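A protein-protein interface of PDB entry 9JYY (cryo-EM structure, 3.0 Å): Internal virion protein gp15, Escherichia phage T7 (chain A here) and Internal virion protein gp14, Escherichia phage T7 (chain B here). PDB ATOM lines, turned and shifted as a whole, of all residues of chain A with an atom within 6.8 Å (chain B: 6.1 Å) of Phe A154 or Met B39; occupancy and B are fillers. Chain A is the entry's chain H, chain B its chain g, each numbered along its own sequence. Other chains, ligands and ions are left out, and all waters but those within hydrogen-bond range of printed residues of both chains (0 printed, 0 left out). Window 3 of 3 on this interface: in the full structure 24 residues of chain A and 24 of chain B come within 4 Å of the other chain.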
ATOM      1  N   LEU A 104      18.450  25.376  -1.427  1.00  0.00           N
ATOM      2  CA  LEU A 104      18.815  24.925  -2.767  1.00  0.00           C
ATOM      3  C   LEU A 104      19.704  23.692  -2.713  1.00  0.00           C
ATOM      4  O   LEU A 104      19.479  22.720  -3.442  1.00  0.00           O
ATOM      5  CB  LEU A 104      19.523  26.044  -3.529  1.00  0.00           C
ATOM      6  CG  LEU A 104      20.242  25.603  -4.808  1.00  0.00           C
ATOM      7  CD1 LEU A 104      19.283  25.475  -5.964  1.00  0.00           C
ATOM      8  CD2 LEU A 104      21.368  26.552  -5.162  1.00  0.00           C
ATOM      9  N   THR A 108      18.655  20.007  -4.085  1.00  0.00           N
ATOM     10  CA  THR A 108      19.455  19.437  -5.160  1.00  0.00           C
ATOM     11  C   THR A 108      20.085  18.118  -4.742  1.00  0.00           C
ATOM     12  O   THR A 108      20.113  17.165  -5.525  1.00  0.00           O
ATOM     13  CB  THR A 108      20.533  20.428  -5.587  1.00  0.00           C
ATOM     14  OG1 THR A 108      19.910  21.639  -6.028  1.00  0.00           O
ATOM     15  CG2 THR A 108      21.368  19.855  -6.717  1.00  0.00           C
ATOM     16  N   LEU A 115      16.634  10.886  -8.071  1.00  0.00           N
ATOM     17  CA  LEU A 115      16.355  10.743  -9.488  1.00  0.00           C
ATOM     18  C   LEU A 115      17.329   9.795 -10.154  1.00  0.00           C
ATOM     19  O   LEU A 115      17.014   8.615 -10.306  1.00  0.00           O
ATOM     20  CB  LEU A 115      16.435  12.106 -10.177  1.00  0.00           C
ATOM     21  CG  LEU A 115      16.575  12.099 -11.700  1.00  0.00           C
ATOM     22  CD1 LEU A 115      15.275  11.708 -12.377  1.00  0.00           C
ATOM     23  CD2 LEU A 115      17.104  13.422 -12.197  1.00  0.00           C
ATOM     24  N   VAL A 149      28.269  13.984 -10.266  1.00  0.00           N
ATOM     25  CA  VAL A 149      27.909  14.586 -11.549  1.00  0.00           C
ATOM     26  C   VAL A 149      26.703  15.510 -11.404  1.00  0.00           C
ATOM     27  O   VAL A 149      26.659  16.582 -12.018  1.00  0.00           O
ATOM     28  CB  VAL A 149      27.689  13.509 -12.630  1.00  0.00           C
ATOM     29  CG1 VAL A 149      28.860  12.547 -12.663  1.00  0.00           C
ATOM     30  CG2 VAL A 149      26.390  12.756 -12.418  1.00  0.00           C
ATOM     31  N   TYR A 150      25.706  15.123 -10.602  1.00  0.00           N
ATOM     32  CA  TYR A 150      24.549  15.984 -10.415  1.00  0.00           C
ATOM     33  C   TYR A 150      24.949  17.283  -9.743  1.00  0.00           C
ATOM     34  O   TYR A 150      24.457  18.356 -10.107  1.00  0.00           O
ATOM     35  CB  TYR A 150      23.480  15.291  -9.576  1.00  0.00           C
ATOM     36  CG  TYR A 150      22.095  15.850  -9.817  1.00  0.00           C
ATOM     37  CD1 TYR A 150      21.487  15.735 -11.052  1.00  0.00           C
ATOM     38  CD2 TYR A 150      21.373  16.433  -8.789  1.00  0.00           C
ATOM     39  CE1 TYR A 150      20.214  16.219 -11.262  1.00  0.00           C
ATOM     40  CE2 TYR A 150      20.111  16.933  -8.994  1.00  0.00           C
ATOM     41  CZ  TYR A 150      19.533  16.825 -10.231  1.00  0.00           C
ATOM     42  OH  TYR A 150      18.267  17.321 -10.429  1.00  0.00           O
ATOM     43  N   ALA A 151      25.835  17.210  -8.745  1.00  0.00           N
ATOM     44  CA  ALA A 151      26.296  18.436  -8.113  1.00  0.00           C
ATOM     45  C   ALA A 151      27.015  19.329  -9.112  1.00  0.00           C
ATOM     46  O   ALA A 151      26.657  20.500  -9.272  1.00  0.00           O
ATOM     47  CB  ALA A 151      27.208  18.109  -6.935  1.00  0.00           C
ATOM     48  N   GLU A 152      28.007  18.787  -9.822  1.00  0.00           N
ATOM     49  CA  GLU A 152      28.820  19.635 -10.687  1.00  0.00           C
ATOM     50  C   GLU A 152      28.003  20.199 -11.844  1.00  0.00           C
ATOM     51  O   GLU A 152      28.280  21.301 -12.329  1.00  0.00           O
ATOM     52  CB  GLU A 152      30.042  18.866 -11.194  1.00  0.00           C
ATOM     53  CG  GLU A 152      29.738  17.638 -12.031  1.00  0.00           C
ATOM     54  CD  GLU A 152      29.534  17.958 -13.497  1.00  0.00           C
ATOM     55  OE1 GLU A 152      29.984  19.039 -13.932  1.00  0.00           O
ATOM     56  OE2 GLU A 152      28.931  17.129 -14.214  1.00  0.00           O
ATOM     57  N   GLN A 153      26.988  19.462 -12.300  1.00  0.00           N
ATOM     58  CA  GLN A 153      26.117  19.993 -13.345  1.00  0.00           C
ATOM     59  C   GLN A 153      25.308  21.176 -12.830  1.00  0.00           C
ATOM     60  O   GLN A 153      24.967  22.088 -13.591  1.00  0.00           O
ATOM     61  CB  GLN A 153      25.199  18.897 -13.877  1.00  0.00           C
ATOM     62  CG  GLN A 153      24.660  19.148 -15.280  1.00  0.00           C
ATOM     63  CD  GLN A 153      25.736  19.428 -16.322  1.00  0.00           C
ATOM     64  OE1 GLN A 153      26.376  20.480 -16.315  1.00  0.00           O
ATOM     65  NE2 GLN A 153      25.929  18.481 -17.233  1.00  0.00           N
ATOM     66  N   PHE A 154      24.977  21.166 -11.545  1.00  0.00           N
ATOM     67  CA  PHE A 154      24.419  22.333 -10.892  1.00  0.00           C
ATOM     68  C   PHE A 154      25.555  23.250 -10.444  1.00  0.00           C
ATOM     69  O   PHE A 154      26.727  23.034 -10.764  1.00  0.00           O
ATOM     70  CB  PHE A 154      23.547  21.904  -9.717  1.00  0.00           C
ATOM     71  CG  PHE A 154      22.096  21.762 -10.063  1.00  0.00           C
ATOM     72  CD1 PHE A 154      21.674  20.782 -10.940  1.00  0.00           C
ATOM     73  CD2 PHE A 154      21.149  22.589  -9.494  1.00  0.00           C
ATOM     74  CE1 PHE A 154      20.341  20.646 -11.256  1.00  0.00           C
ATOM     75  CE2 PHE A 154      19.815  22.449  -9.807  1.00  0.00           C
ATOM     76  CZ  PHE A 154      19.412  21.479 -10.689  1.00  0.00           C
ATOM     77  N   GLY A 155      25.212  24.297  -9.698  1.00  0.00           N
ATOM     78  CA  GLY A 155      26.247  25.157  -9.151  1.00  0.00           C
ATOM     79  C   GLY A 155      26.931  24.553  -7.940  1.00  0.00           C
ATOM     80  O   GLY A 155      28.032  24.963  -7.566  1.00  0.00           O
ATOM     81  N   ILE A 156      26.292  23.568  -7.312  1.00  0.00           N
ATOM     82  CA  ILE A 156      26.756  23.059  -6.030  1.00  0.00           C
ATOM     83  C   ILE A 156      28.006  22.213  -6.230  1.00  0.00           C
ATOM     84  O   ILE A 156      28.143  21.503  -7.233  1.00  0.00           O
ATOM     85  CB  ILE A 156      25.642  22.250  -5.342  1.00  0.00           C
ATOM     86  CG1 ILE A 156      24.430  23.131  -5.035  1.00  0.00           C
ATOM     87  CG2 ILE A 156      26.146  21.623  -4.059  1.00  0.00           C
ATOM     88  CD1 ILE A 156      23.412  23.201  -6.148  1.00  0.00           C
ATOM     89  N   ASP A 157      28.934  22.295  -5.279  1.00  0.00           N
ATOM     90  CA  ASP A 157      30.085  21.408  -5.271  1.00  0.00           C
ATOM     91  C   ASP A 157      29.877  20.294  -4.260  1.00  0.00           C
ATOM     92  O   ASP A 157      29.552  20.572  -3.098  1.00  0.00           O
ATOM     93  CB  ASP A 157      31.366  22.181  -4.950  1.00  0.00           C
ATOM     94  CG  ASP A 157      31.907  22.936  -6.153  1.00  0.00           C
ATOM     95  OD1 ASP A 157      31.495  22.621  -7.288  1.00  0.00           O
ATOM     96  OD2 ASP A 157      32.741  23.847  -5.964  1.00  0.00           O
ATOM     97  N   TYR A 163      24.591  19.787   0.925  1.00  0.00           N
ATOM     98  CA  TYR A 163      24.358  18.896  -0.204  1.00  0.00           C
ATOM     99  C   TYR A 163      24.362  17.437   0.230  1.00  0.00           C
ATOM    100  O   TYR A 163      23.504  16.660  -0.196  1.00  0.00           O
ATOM    101  CB  TYR A 163      25.395  19.132  -1.296  1.00  0.00           C
ATOM    102  CG  TYR A 163      25.144  18.315  -2.538  1.00  0.00           C
ATOM    103  CD1 TYR A 163      24.217  18.722  -3.483  1.00  0.00           C
ATOM    104  CD2 TYR A 163      25.832  17.136  -2.768  1.00  0.00           C
ATOM    105  CE1 TYR A 163      23.988  17.979  -4.619  1.00  0.00           C
ATOM    106  CE2 TYR A 163      25.607  16.389  -3.901  1.00  0.00           C
ATOM    107  CZ  TYR A 163      24.685  16.815  -4.822  1.00  0.00           C
ATOM    108  OH  TYR A 163      24.458  16.068  -5.951  1.00  0.00           O
ATOM    109  N   GLY B  34      19.287  12.116 -21.935  1.00  0.00           N
ATOM    110  CA  GLY B  34      18.130  12.978 -21.773  1.00  0.00           C
ATOM    111  C   GLY B  34      18.271  13.917 -20.594  1.00  0.00           C
ATOM    112  O   GLY B  34      17.951  15.103 -20.692  1.00  0.00           O
ATOM    113  N   ARG B  35      18.768  13.406 -19.467  1.00  0.00           N
ATOM    114  CA  ARG B  35      18.980  14.276 -18.311  1.00  0.00           C
ATOM    115  C   ARG B  35      20.053  15.321 -18.589  1.00  0.00           C
ATOM    116  O   ARG B  35      19.933  16.474 -18.156  1.00  0.00           O
ATOM    117  CB  ARG B  35      19.338  13.450 -17.081  1.00  0.00           C
ATOM    118  CG  ARG B  35      18.175  12.671 -16.534  1.00  0.00           C
ATOM    119  CD  ARG B  35      18.643  11.562 -15.641  1.00  0.00           C
ATOM    120  NE  ARG B  35      17.536  10.705 -15.244  1.00  0.00           N
ATOM    121  CZ  ARG B  35      17.687   9.531 -14.652  1.00  0.00           C
ATOM    122  NH1 ARG B  35      18.885   9.046 -14.380  1.00  0.00           N
ATOM    123  NH2 ARG B  35      16.609   8.821 -14.340  1.00  0.00           N
ATOM    124  N   ARG B  36      21.115  14.939 -19.298  1.00  0.00           N
ATOM    125  CA  ARG B  36      22.152  15.910 -19.632  1.00  0.00           C
ATOM    126  C   ARG B  36      21.610  17.009 -20.539  1.00  0.00           C
ATOM    127  O   ARG B  36      21.913  18.194 -20.348  1.00  0.00           O
ATOM    128  CB  ARG B  36      23.340  15.203 -20.280  1.00  0.00           C
ATOM    129  CG  ARG B  36      24.249  16.107 -21.082  1.00  0.00           C
ATOM    130  CD  ARG B  36      24.824  15.352 -22.262  1.00  0.00           C
ATOM    131  NE  ARG B  36      23.783  14.697 -23.043  1.00  0.00           N
ATOM    132  CZ  ARG B  36      23.173  15.243 -24.085  1.00  0.00           C
ATOM    133  NH1 ARG B  36      23.489  16.454 -24.514  1.00  0.00           N
ATOM    134  NH2 ARG B  36      22.229  14.554 -24.718  1.00  0.00           N
ATOM    135  N   GLN B  37      20.793  16.640 -21.525  1.00  0.00           N
ATOM    136  CA  GLN B  37      20.231  17.651 -22.410  1.00  0.00           C
ATOM    137  C   GLN B  37      19.218  18.514 -21.672  1.00  0.00           C
ATOM    138  O   GLN B  37      19.079  19.705 -21.963  1.00  0.00           O
ATOM    139  CB  GLN B  37      19.630  16.985 -23.652  1.00  0.00           C
ATOM    140  CG  GLN B  37      18.214  16.433 -23.525  1.00  0.00           C
ATOM    141  CD  GLN B  37      17.148  17.484 -23.752  1.00  0.00           C
ATOM    142  OE1 GLN B  37      17.356  18.436 -24.501  1.00  0.00           O
ATOM    143  NE2 GLN B  37      16.002  17.316 -23.106  1.00  0.00           N
ATOM    144  N   ALA B  38      18.511  17.941 -20.696  1.00  0.00           N
ATOM    145  CA  ALA B  38      17.619  18.748 -19.870  1.00  0.00           C
ATOM    146  C   ALA B  38      18.404  19.757 -19.045  1.00  0.00           C
ATOM    147  O   ALA B  38      17.972  20.902 -18.870  1.00  0.00           O
ATOM    148  CB  ALA B  38      16.783  17.847 -18.966  1.00  0.00           C
ATOM    149  N   MET B  39      19.561  19.347 -18.526  1.00  0.00           N
ATOM    150  CA  MET B  39      20.440  20.286 -17.840  1.00  0.00           C
ATOM    151  C   MET B  39      20.895  21.397 -18.776  1.00  0.00           C
ATOM    152  O   MET B  39      20.970  22.568 -18.381  1.00  0.00           O
ATOM    153  CB  MET B  39      21.648  19.545 -17.283  1.00  0.00           C
ATOM    154  CG  MET B  39      21.327  18.615 -16.153  1.00  0.00           C
ATOM    155  SD  MET B  39      21.014  19.539 -14.649  1.00  0.00           S
ATOM    156  CE  MET B  39      21.513  18.314 -13.463  1.00  0.00           C
ATOM    157  N   GLU B  40      21.228  21.036 -20.016  1.00  0.00           N
ATOM    158  CA  GLU B  40      21.582  22.032 -21.023  1.00  0.00           C
ATOM    159  C   GLU B  40      20.451  23.029 -21.233  1.00  0.00           C
ATOM    160  O   GLU B  40      20.677  24.247 -21.242  1.00  0.00           O
ATOM    161  CB  GLU B  40      21.931  21.321 -22.329  1.00  0.00           C
ATOM    162  CG  GLU B  40      22.527  22.184 -23.431  1.00  0.00           C
ATOM    163  CD  GLU B  40      21.464  22.884 -24.263  1.00  0.00           C
ATOM    164  OE1 GLU B  40      20.344  22.343 -24.366  1.00  0.00           O
ATOM    165  OE2 GLU B  40      21.755  23.951 -24.841  1.00  0.00           O
ATOM    166  N   ILE B  41      19.225  22.531 -21.384  1.00  0.00           N
ATOM    167  CA  ILE B  41      18.074  23.413 -21.565  1.00  0.00           C
ATOM    168  C   ILE B  41      17.911  24.331 -20.365  1.00  0.00           C
ATOM    169  O   ILE B  41      17.643  25.528 -20.509  1.00  0.00           O
ATOM    170  CB  ILE B  41      16.795  22.598 -21.815  1.00  0.00           C
ATOM    171  CG1 ILE B  41      16.975  21.640 -22.990  1.00  0.00           C
ATOM    172  CG2 ILE B  41      15.642  23.523 -22.047  1.00  0.00           C
ATOM    173  CD1 ILE B  41      15.724  20.870 -23.327  1.00  0.00           C
ATOM    174  N   MET B  42      18.055  23.780 -19.160  1.00  0.00           N
ATOM    175  CA  MET B  42      17.919  24.593 -17.958  1.00  0.00           C
ATOM    176  C   MET B  42      18.943  25.719 -17.940  1.00  0.00           C
ATOM    177  O   MET B  42      18.611  26.872 -17.647  1.00  0.00           O
ATOM    178  CB  MET B  42      18.072  23.725 -16.713  1.00  0.00           C
ATOM    179  CG  MET B  42      17.912  24.498 -15.420  1.00  0.00           C
ATOM    180  SD  MET B  42      18.506  23.626 -13.963  1.00  0.00           S
ATOM    181  CE  MET B  42      20.107  23.070 -14.530  1.00  0.00           C
ATOM    182  N   ARG B  43      20.200  25.401 -18.250  1.00  0.00           N
ATOM    183  CA  ARG B  43      21.245  26.417 -18.162  1.00  0.00           C
ATOM    184  C   ARG B  43      21.077  27.489 -19.231  1.00  0.00           C
ATOM    185  O   ARG B  43      21.259  28.679 -18.954  1.00  0.00           O
ATOM    186  CB  ARG B  43      22.625  25.773 -18.258  1.00  0.00           C
ATOM    187  CG  ARG B  43      22.980  24.905 -17.071  1.00  0.00           C
ATOM    188  CD  ARG B  43      24.322  24.242 -17.280  1.00  0.00           C
ATOM    189  NE  ARG B  43      24.335  23.430 -18.489  1.00  0.00           N
ATOM    190  CZ  ARG B  43      25.378  22.727 -18.906  1.00  0.00           C
ATOM    191  NH1 ARG B  43      26.515  22.712 -18.231  1.00  0.00           N
ATOM    192  NH2 ARG B  43      25.274  22.015 -20.025  1.00  0.00           N
ATOM    193  N   GLN B  44      20.739  27.096 -20.459  1.00  0.00           N
ATOM    194  CA  GLN B  44      20.633  28.089 -21.525  1.00  0.00           C
ATOM    195  C   GLN B  44      19.348  28.902 -21.416  1.00  0.00           C
ATOM    196  O   GLN B  44      19.350  30.116 -21.645  1.00  0.00           O
ATOM    197  CB  GLN B  44      20.737  27.415 -22.892  1.00  0.00           C
ATOM    198  CG  GLN B  44      21.884  26.407 -23.073  1.00  0.00           C
ATOM    199  CD  GLN B  44      23.204  26.753 -22.378  1.00  0.00           C
ATOM    200  OE1 GLN B  44      23.481  27.904 -22.036  1.00  0.00           O
ATOM    201  NE2 GLN B  44      24.022  25.731 -22.156  1.00  0.00           N
ATOM    202  N   ALA B  63      12.415  20.010 -19.130  1.00  0.00           N
ATOM    203  CA  ALA B  63      13.549  19.782 -18.245  1.00  0.00           C
ATOM    204  C   ALA B  63      13.083  19.286 -16.885  1.00  0.00           C
ATOM    205  O   ALA B  63      13.631  18.321 -16.343  1.00  0.00           O
ATOM    206  CB  ALA B  63      14.369  21.061 -18.102  1.00  0.00           C
ATOM    207  N   LEU B  67      13.926  15.709 -15.104  1.00  0.00           N
ATOM    208  CA  LEU B  67      14.624  15.651 -13.821  1.00  0.00           C
ATOM    209  C   LEU B  67      13.747  15.051 -12.729  1.00  0.00           C
ATOM    210  O   LEU B  67      14.227  14.787 -11.621  1.00  0.00           O
ATOM    211  CB  LEU B  67      15.119  17.037 -13.410  1.00  0.00           C
ATOM    212  CG  LEU B  67      16.448  17.545 -13.975  1.00  0.00           C
ATOM    213  CD1 LEU B  67      17.573  16.670 -13.491  1.00  0.00           C
ATOM    214  CD2 LEU B  67      16.465  17.570 -15.474  1.00  0.00           C
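The side-chain amide oxygen (OE1) of Gln A153 sits at hydrogen-bond distance from the guanidinium group (NH1) of Arg B43 (2.9 Å).
The backbone carbonyl oxygen (O) of Met B39 lies close to the guanidinium group (NE) of Arg B43 (3.5 Å).
Among the printed residues, pairs that only touch across the chains: Leu A115 with Arg B35, Leu A115 with Leu B67, Tyr A150 with Met B39, Tyr A150 with Leu B67, Gln A153 with Met B39 and Phe A154 with Met B39.
Of the printed residues of chain A, Arg B35 touches Leu A115 (3.7 Å).
Met B39 touches just these residues of chain A: Tyr A150, Gln A153 and Phe A154.
Of the printed residues of chain A, Arg B43 touches Gln A153.
Of the 13 printed residues of chain A, 4 touch a printed residue of chain B.
Hydrophobic or aromatic side chains of chain A that line the printed part of chain B: Leu A115, Tyr A150 and Phe A154.
Of the 13 printed residues of chain B, 4 touch a printed residue of chain A.
Among the printed residues, 7 pairs touch across the chains.
Among the printed residues, no Asp or Glu carboxylate lies within 4 Å of a Lys or Arg side-chain nitrogen of the other chain.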
